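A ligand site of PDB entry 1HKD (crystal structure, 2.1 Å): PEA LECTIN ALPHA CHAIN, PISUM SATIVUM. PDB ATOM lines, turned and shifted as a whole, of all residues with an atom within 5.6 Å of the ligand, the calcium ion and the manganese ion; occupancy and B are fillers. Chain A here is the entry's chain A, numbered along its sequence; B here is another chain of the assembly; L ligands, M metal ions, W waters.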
ATOM      1  N   ALA A  80      10.997   1.936  23.050  1.00  0.00           N
ATOM      2  CA  ALA A  80      12.138   2.837  22.872  1.00  0.00           C
ATOM      3  C   ALA A  80      13.450   2.153  23.284  1.00  0.00           C
ATOM      4  O   ALA A  80      13.395   1.127  23.951  1.00  0.00           O
ATOM      5  CB  ALA A  80      11.950   4.094  23.686  1.00  0.00           C
ATOM      6  N   ASP A  81      14.594   2.574  22.747  1.00  0.00           N
ATOM      7  CA  ASP A  81      14.723   3.633  21.751  1.00  0.00           C
ATOM      8  C   ASP A  81      15.051   3.001  20.402  1.00  0.00           C
ATOM      9  O   ASP A  81      14.811   3.548  19.330  1.00  0.00           O
ATOM     10  CB  ASP A  81      15.903   4.493  22.137  1.00  0.00           C
ATOM     11  CG  ASP A  81      15.501   5.592  23.042  1.00  0.00           C
ATOM     12  OD1 ASP A  81      15.832   5.527  24.244  1.00  0.00           O
ATOM     13  OD2 ASP A  81      14.816   6.546  22.643  1.00  0.00           O
ATOM     14  N   GLY A  97      23.263   7.952  25.618  1.00  0.00           N
ATOM     15  CA  GLY A  97      22.200   6.968  25.584  1.00  0.00           C
ATOM     16  C   GLY A  97      20.883   7.520  25.075  1.00  0.00           C
ATOM     17  O   GLY A  97      20.860   8.519  24.340  1.00  0.00           O
ATOM     18  N   GLY A  98      19.774   6.868  25.458  1.00  0.00           N
ATOM     19  CA  GLY A  98      18.444   7.270  25.049  1.00  0.00           C
ATOM     20  C   GLY A  98      18.287   7.274  23.530  1.00  0.00           C
ATOM     21  O   GLY A  98      18.719   6.336  22.843  1.00  0.00           O
ATOM     22  N   GLY A  99      17.673   8.350  23.011  1.00  0.00           N
ATOM     23  CA  GLY A  99      17.442   8.519  21.580  1.00  0.00           C
ATOM     24  C   GLY A  99      18.713   8.609  20.725  1.00  0.00           C
ATOM     25  O   GLY A  99      18.637   8.546  19.499  1.00  0.00           O
ATOM     26  N   TYR A 100      19.859   8.780  21.380  1.00  0.00           N
ATOM     27  CA  TYR A 100      21.136   8.848  20.689  1.00  0.00           C
ATOM     28  C   TYR A 100      21.706   7.445  20.431  1.00  0.00           C
ATOM     29  O   TYR A 100      22.767   7.295  19.827  1.00  0.00           O
ATOM     30  CB  TYR A 100      22.132   9.722  21.472  1.00  0.00           C
ATOM     31  CG  TYR A 100      21.730  11.176  21.506  1.00  0.00           C
ATOM     32  CD1 TYR A 100      22.008  12.013  20.432  1.00  0.00           C
ATOM     33  CD2 TYR A 100      20.987  11.686  22.561  1.00  0.00           C
ATOM     34  CE1 TYR A 100      21.619  13.368  20.456  1.00  0.00           C
ATOM     35  CE2 TYR A 100      20.595  13.007  22.595  1.00  0.00           C
ATOM     36  CZ  TYR A 100      20.914  13.841  21.542  1.00  0.00           C
ATOM     37  OH  TYR A 100      20.527  15.153  21.604  1.00  0.00           O
ATOM     38  N   GLU A 119      20.496   2.389  11.908  1.00  0.00           N
ATOM     39  CA  GLU A 119      19.606   2.348  13.048  1.00  0.00           C
ATOM     40  C   GLU A 119      18.266   1.703  12.754  1.00  0.00           C
ATOM     41  O   GLU A 119      17.775   1.739  11.640  1.00  0.00           O
ATOM     42  CB  GLU A 119      19.385   3.771  13.590  1.00  0.00           C
ATOM     43  CG  GLU A 119      18.762   4.720  12.578  1.00  0.00           C
ATOM     44  CD  GLU A 119      18.299   6.015  13.202  1.00  0.00           C
ATOM     45  OE1 GLU A 119      17.132   6.386  13.003  1.00  0.00           O
ATOM     46  OE2 GLU A 119      19.090   6.632  13.949  1.00  0.00           O
ATOM     47  N   ASP A 121      15.155   2.427  14.623  1.00  0.00           N
ATOM     48  CA  ASP A 121      14.611   3.381  15.574  1.00  0.00           C
ATOM     49  C   ASP A 121      13.139   3.139  15.913  1.00  0.00           C
ATOM     50  O   ASP A 121      12.283   3.280  15.053  1.00  0.00           O
ATOM     51  CB  ASP A 121      14.800   4.789  14.997  1.00  0.00           C
ATOM     52  CG  ASP A 121      14.721   5.877  16.037  1.00  0.00           C
ATOM     53  OD1 ASP A 121      14.079   5.681  17.105  1.00  0.00           O
ATOM     54  OD2 ASP A 121      15.271   6.982  15.839  1.00  0.00           O
ATOM     55  N   THR A 122      12.853   2.887  17.193  1.00  0.00           N
ATOM     56  CA  THR A 122      11.482   2.603  17.613  1.00  0.00           C
ATOM     57  C   THR A 122      10.768   3.752  18.313  1.00  0.00           C
ATOM     58  O   THR A 122       9.596   3.605  18.691  1.00  0.00           O
ATOM     59  CB  THR A 122      11.456   1.389  18.581  1.00  0.00           C
ATOM     60  OG1 THR A 122      12.403   1.613  19.641  1.00  0.00           O
ATOM     61  CG2 THR A 122      11.921   0.121  17.888  1.00  0.00           C
ATOM     62  N   PHE A 123      11.471   4.849  18.555  1.00  0.00           N
ATOM     63  CA  PHE A 123      10.874   5.971  19.274  1.00  0.00           C
ATOM     64  C   PHE A 123      11.119   7.296  18.578  1.00  0.00           C
ATOM     65  O   PHE A 123      12.260   7.668  18.311  1.00  0.00           O
ATOM     66  CB  PHE A 123      11.404   6.013  20.729  1.00  0.00           C
ATOM     67  CG  PHE A 123      10.834   7.127  21.566  1.00  0.00           C
ATOM     68  CD1 PHE A 123      11.434   8.371  21.592  1.00  0.00           C
ATOM     69  CD2 PHE A 123       9.727   6.906  22.388  1.00  0.00           C
ATOM     70  CE1 PHE A 123      10.909   9.415  22.349  1.00  0.00           C
ATOM     71  CE2 PHE A 123       9.197   7.938  23.163  1.00  0.00           C
ATOM     72  CZ  PHE A 123       9.786   9.185  23.138  1.00  0.00           C
ATOM     73  N   TYR A 124      10.024   8.009  18.327  1.00  0.00           N
ATOM     74  CA  TYR A 124      10.051   9.311  17.684  1.00  0.00           C
ATOM     75  C   TYR A 124      10.598  10.430  18.591  1.00  0.00           C
ATOM     76  O   TYR A 124       9.941  10.826  19.554  1.00  0.00           O
ATOM     77  CB  TYR A 124       8.630   9.688  17.211  1.00  0.00           C
ATOM     78  CG  TYR A 124       8.480  11.126  16.736  1.00  0.00           C
ATOM     79  CD1 TYR A 124       9.116  11.569  15.585  1.00  0.00           C
ATOM     80  CD2 TYR A 124       7.718  12.046  17.467  1.00  0.00           C
ATOM     81  CE1 TYR A 124       8.993  12.883  15.143  1.00  0.00           C
ATOM     82  CE2 TYR A 124       7.577  13.374  17.030  1.00  0.00           C
ATOM     83  CZ  TYR A 124       8.218  13.776  15.863  1.00  0.00           C
ATOM     84  OH  TYR A 124       8.100  15.076  15.419  1.00  0.00           O
ATOM     85  N   ASN A 125      11.787  10.936  18.263  1.00  0.00           N
ATOM     86  CA  ASN A 125      12.383  12.067  18.964  1.00  0.00           C
ATOM     87  C   ASN A 125      12.106  13.294  18.106  1.00  0.00           C
ATOM     88  O   ASN A 125      12.670  13.423  17.021  1.00  0.00           O
ATOM     89  CB  ASN A 125      13.890  11.869  19.134  1.00  0.00           C
ATOM     90  CG  ASN A 125      14.244  10.736  20.075  1.00  0.00           C
ATOM     91  OD1 ASN A 125      14.374   9.595  19.661  1.00  0.00           O
ATOM     92  ND2 ASN A 125      14.442  11.060  21.351  1.00  0.00           N
ATOM     93  N   TRP A 128      14.705  15.582  15.861  1.00  0.00           N
ATOM     94  CA  TRP A 128      15.424  15.139  14.661  1.00  0.00           C
ATOM     95  C   TRP A 128      14.803  14.004  13.823  1.00  0.00           C
ATOM     96  O   TRP A 128      15.146  13.856  12.651  1.00  0.00           O
ATOM     97  CB  TRP A 128      16.878  14.778  15.016  1.00  0.00           C
ATOM     98  CG  TRP A 128      16.985  13.603  15.963  1.00  0.00           C
ATOM     99  CD1 TRP A 128      16.745  12.294  15.668  1.00  0.00           C
ATOM    100  CD2 TRP A 128      17.233  13.659  17.364  1.00  0.00           C
ATOM    101  NE1 TRP A 128      16.878  11.513  16.801  1.00  0.00           N
ATOM    102  CE2 TRP A 128      17.184  12.333  17.861  1.00  0.00           C
ATOM    103  CE3 TRP A 128      17.543  14.682  18.258  1.00  0.00           C
ATOM    104  CZ2 TRP A 128      17.401  12.020  19.197  1.00  0.00           C
ATOM    105  CZ3 TRP A 128      17.767  14.373  19.586  1.00  0.00           C
ATOM    106  CH2 TRP A 128      17.673  13.050  20.047  1.00  0.00           C
ATOM    107  N   ASP A 129      13.896  13.216  14.401  1.00  0.00           N
ATOM    108  CA  ASP A 129      13.305  12.094  13.652  1.00  0.00           C
ATOM    109  C   ASP A 129      12.261  12.524  12.629  1.00  0.00           C
ATOM    110  O   ASP A 129      11.659  13.588  12.764  1.00  0.00           O
ATOM    111  CB  ASP A 129      12.713  11.077  14.619  1.00  0.00           C
ATOM    112  CG  ASP A 129      13.761  10.169  15.230  1.00  0.00           C
ATOM    113  OD1 ASP A 129      14.785   9.889  14.572  1.00  0.00           O
ATOM    114  OD2 ASP A 129      13.602   9.651  16.363  1.00  0.00           O
ATOM    115  N   PRO A 130      11.990  11.660  11.648  1.00  0.00           N
ATOM    116  CA  PRO A 130      10.993  11.951  10.598  1.00  0.00           C
ATOM    117  C   PRO A 130       9.668  12.406  11.205  1.00  0.00           C
ATOM    118  O   PRO A 130       9.123  11.707  12.058  1.00  0.00           O
ATOM    119  CB  PRO A 130      10.843  10.601   9.895  1.00  0.00           C
ATOM    120  CG  PRO A 130      12.190   9.953  10.059  1.00  0.00           C
ATOM    121  CD  PRO A 130      12.585  10.326  11.460  1.00  0.00           C
ATOM    122  N   HIS A 136      11.360   3.571  12.190  1.00  0.00           N
ATOM    123  CA  HIS A 136      12.041   3.570  10.904  1.00  0.00           C
ATOM    124  C   HIS A 136      13.432   3.010  10.952  1.00  0.00           C
ATOM    125  O   HIS A 136      14.046   2.899  12.010  1.00  0.00           O
ATOM    126  CB  HIS A 136      12.139   5.022  10.410  1.00  0.00           C
ATOM    127  CG  HIS A 136      12.689   5.971  11.436  1.00  0.00           C
ATOM    128  ND1 HIS A 136      11.942   6.431  12.506  1.00  0.00           N
ATOM    129  CD2 HIS A 136      13.945   6.471  11.614  1.00  0.00           C
ATOM    130  CE1 HIS A 136      12.698   7.184  13.276  1.00  0.00           C
ATOM    131  NE2 HIS A 136      13.918   7.225  12.762  1.00  0.00           N
ATOM    132  N   ILE A 144      22.931  11.716  14.695  1.00  0.00           N
ATOM    133  CA  ILE A 144      21.725  10.944  15.022  1.00  0.00           C
ATOM    134  C   ILE A 144      20.595  11.237  14.026  1.00  0.00           C
ATOM    135  O   ILE A 144      19.597  10.521  13.953  1.00  0.00           O
ATOM    136  CB  ILE A 144      21.278  11.185  16.472  1.00  0.00           C
ATOM    137  CG1 ILE A 144      20.301  10.089  16.939  1.00  0.00           C
ATOM    138  CG2 ILE A 144      20.653  12.569  16.658  1.00  0.00           C
ATOM    139  CD1 ILE A 144      20.883   8.670  16.867  1.00  0.00           C
ATOM    140  N   SER A 146      19.432  10.943  10.585  1.00  0.00           N
ATOM    141  CA  SER A 146      19.763  10.131   9.419  1.00  0.00           C
ATOM    142  C   SER A 146      19.838  10.863   8.075  1.00  0.00           C
ATOM    143  O   SER A 146      19.112  11.822   7.840  1.00  0.00           O
ATOM    144  CB  SER A 146      18.784   8.948   9.304  1.00  0.00           C
ATOM    145  OG  SER A 146      18.555   8.336  10.572  1.00  0.00           O
ATOM    146  N   THR A 149      15.971   7.536   5.537  1.00  0.00           N
ATOM    147  CA  THR A 149      15.196   6.648   6.393  1.00  0.00           C
ATOM    148  C   THR A 149      14.134   5.913   5.592  1.00  0.00           C
ATOM    149  O   THR A 149      13.830   6.278   4.445  1.00  0.00           O
ATOM    150  CB  THR A 149      14.477   7.441   7.509  1.00  0.00           C
ATOM    151  OG1 THR A 149      13.683   8.496   6.922  1.00  0.00           O
ATOM    152  CG2 THR A 149      15.465   8.164   8.409  1.00  0.00           C
ATOM    153  N   THR B  28      17.590   2.408  25.935  1.00  0.00           N
ATOM    154  CA  THR B  28      16.233   2.691  26.389  1.00  0.00           C
ATOM    155  C   THR B  28      16.298   4.028  27.110  1.00  0.00           C
ATOM    156  O   THR B  28      17.380   4.494  27.474  1.00  0.00           O
ATOM    157  CB  THR B  28      15.738   1.625  27.360  1.00  0.00           C
ATOM    158  OG1 THR B  28      16.659   1.533  28.469  1.00  0.00           O
ATOM    159  CG2 THR B  28      15.774   0.245  26.720  1.00  0.00           C
ATOM    160  N   GLY B  29      15.154   4.664  27.286  1.00  0.00           N
ATOM    161  CA  GLY B  29      15.102   5.937  27.987  1.00  0.00           C
ATOM    162  C   GLY B  29      13.923   5.900  28.920  1.00  0.00           C
ATOM    163  O   GLY B  29      13.801   4.966  29.715  1.00  0.00           O
ATOM    164  N   ALA B  30      13.016   6.866  28.785  1.00  0.00           N
ATOM    165  CA  ALA B  30      11.806   6.895  29.611  1.00  0.00           C
ATOM    166  C   ALA B  30      10.926   5.697  29.236  1.00  0.00           C
ATOM    167  O   ALA B  30      10.153   5.224  30.042  1.00  0.00           O
ATOM    168  CB  ALA B  30      11.052   8.212  29.412  1.00  0.00           C
ATOM    169  N   GLU B  31      11.052   5.232  27.991  1.00  0.00           N
ATOM    170  CA  GLU B  31      10.326   4.047  27.517  1.00  0.00           C
ATOM    171  C   GLU B  31      11.374   2.993  27.181  1.00  0.00           C
ATOM    172  O   GLU B  31      12.540   3.331  26.948  1.00  0.00           O
ATOM    173  CB  GLU B  31       9.433   4.378  26.323  1.00  0.00           C
ATOM    174  CG  GLU B  31       8.272   5.299  26.693  1.00  0.00           C
ATOM    175  CD  GLU B  31       7.511   5.804  25.486  1.00  0.00           C
ATOM    176  OE1 GLU B  31       7.388   5.066  24.498  1.00  0.00           O
ATOM    177  OE2 GLU B  31       7.027   6.956  25.542  1.00  0.00           O
ATOM    178  N   TYR B  32      10.967   1.731  27.117  1.00  0.00           N
ATOM    179  CA  TYR B  32      11.968   0.678  26.952  1.00  0.00           C
ATOM    180  C   TYR B  32      11.511  -0.572  26.230  1.00  0.00           C
ATOM    181  O   TYR B  32      10.351  -0.720  25.840  1.00  0.00           O
ATOM    182  CB  TYR B  32      12.455   0.261  28.345  1.00  0.00           C
ATOM    183  CG  TYR B  32      11.318  -0.189  29.240  1.00  0.00           C
ATOM    184  CD1 TYR B  32      10.476   0.734  29.847  1.00  0.00           C
ATOM    185  CD2 TYR B  32      11.003  -1.538  29.369  1.00  0.00           C
ATOM    186  CE1 TYR B  32       9.398   0.332  30.620  1.00  0.00           C
ATOM    187  CE2 TYR B  32       9.945  -1.964  30.147  1.00  0.00           C
ATOM    188  CZ  TYR B  32       9.142  -1.023  30.782  1.00  0.00           C
ATOM    189  OH  TYR B  32       8.082  -1.439  31.550  1.00  0.00           O
HETATM  190  C1  LIG L   1      13.429  10.528  26.987  1.00  0.00           C
HETATM  191  C2  LIG L   1      14.894  10.686  26.574  1.00  0.00           C
HETATM  192  C3  LIG L   1      15.065  10.438  25.077  1.00  0.00           C
HETATM  193  C4  LIG L   1      14.471   9.081  24.705  1.00  0.00           C
HETATM  194  C5  LIG L   1      13.048   8.946  25.223  1.00  0.00           C
HETATM  195  C6  LIG L   1      12.490   7.555  24.965  1.00  0.00           C
HETATM  196  C7  LIG L   1      11.259  11.541  26.878  1.00  0.00           C
HETATM  197  O1  LIG L   1      12.608  11.546  26.374  1.00  0.00           O
HETATM  198  O2  LIG L   1      15.375  11.999  26.897  1.00  0.00           O
HETATM  199  O3  LIG L   1      16.467  10.475  24.747  1.00  0.00           O
HETATM  200  O4  LIG L   1      14.460   8.982  23.278  1.00  0.00           O
HETATM  201  O5  LIG L   1      12.969   9.221  26.629  1.00  0.00           O
HETATM  202  O6  LIG L   1      13.154   6.610  25.802  1.00  0.00           O
HETATM  203 CA    CA M   1      14.476   8.002  17.930  1.00  0.00          CA
HETATM  204 MN    MN M   2      15.832   8.059  13.858  1.00  0.00          MN
HETATM  205  O   HOH W   1      17.852   8.708  14.829  1.00  0.00           O
HETATM  206  O   HOH W   2      17.034  13.400  24.151  1.00  0.00           O
HETATM  207  O   HOH W   3      14.880   6.475  19.671  1.00  0.00           O
HETATM  208  O   HOH W   4      16.484   9.123  11.992  1.00  0.00           O
HETATM  209  O   HOH W   5      16.781   8.414  17.665  1.00  0.00           O
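An oxygen (O4) of the ligand sits at hydrogen-bond distance from the side-chain amide nitrogen of Asn 125.
O4 of the ligand sits at hydrogen-bond distance from OD2 of Asp 81, at 2.5 Å.
The backbone NH of Gly 99 sits at hydrogen-bond distance from an oxygen (O3) of the ligand (3.0 Å).
An oxygen (O6) of the ligand sits at hydrogen-bond distance from the backbone NH (N) of Ala 30 of chain B (3.0 Å).
The backbone NH of Gly 29 of chain B lies close to an oxygen (O6) of the ligand (3.2 Å).
N of Glu 31 of chain B is in hydrogen-bond range of O6 of the ligand, at 3.3 Å.
The side-chain carboxylate (OD1) of Asp 129 sits close to the indole nitrogen (NE1) of Trp 128, 3.5 Å away.
The side-chain hydroxyl (OG) of Ser 146 sits close to the side-chain carboxylate (OE1) of Glu 119 (3.4 Å).
The side-chain carboxylate (OD2) of Asp 81 sits at hydrogen-bond distance from the backbone NH (N) of Gly 99.
The side-chain carboxylate (OD1) of Asp 81 is in hydrogen-bond range of the backbone NH (N) of Gly 29 of chain B (3.2 Å).
N of Thr 122 lies within hydrogen-bond range of O of Asp 81, 3.0 Å away.
Residues that only touch the ligand: Ala 80 (3.5 Å) and Gly 98 (3.8 Å).
Of the 24 residues printed, 4 come within 4 Å of the calcium ion.
The nearest printed residue that does not touch the manganese ion is Ser 146 (4.3 Å).
The calcium ion is bound by the backbone carbonyl oxygen (O) of Phe 123, water W3, the side-chain amide oxygen (OD1) of Asn 125, water W5, the side-chain carboxylate (OD2) of Asp 129, the side-chain carboxylate (OD2) of Asp 121 and the side-chain carboxylate (OD1) of Asp 121.
The calcium ion has seven donor atoms within binding distance.
The manganese ion is bound by the side-chain carboxylate of Asp 129 (2.2 Å), water W4 (2.2 Å), the side-chain carboxylate of Glu 119 (2.3 Å), the side-chain carboxylate of Asp 121 (2.3 Å), water W1 (2.3 Å) and a ring nitrogen (NE2) of His 136 (2.4 Å).
The manganese ion has six donor atoms within binding distance.
Water W5 lies within hydrogen-bond range of O of Gly 99 (2.6 Å) and NE1 of Trp 128 (3.2 Å).
Water W1 bridges the side-chain carboxylate of Glu 119 (2.6 Å) and the backbone carbonyl oxygen of Ile 144 (2.7 Å).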
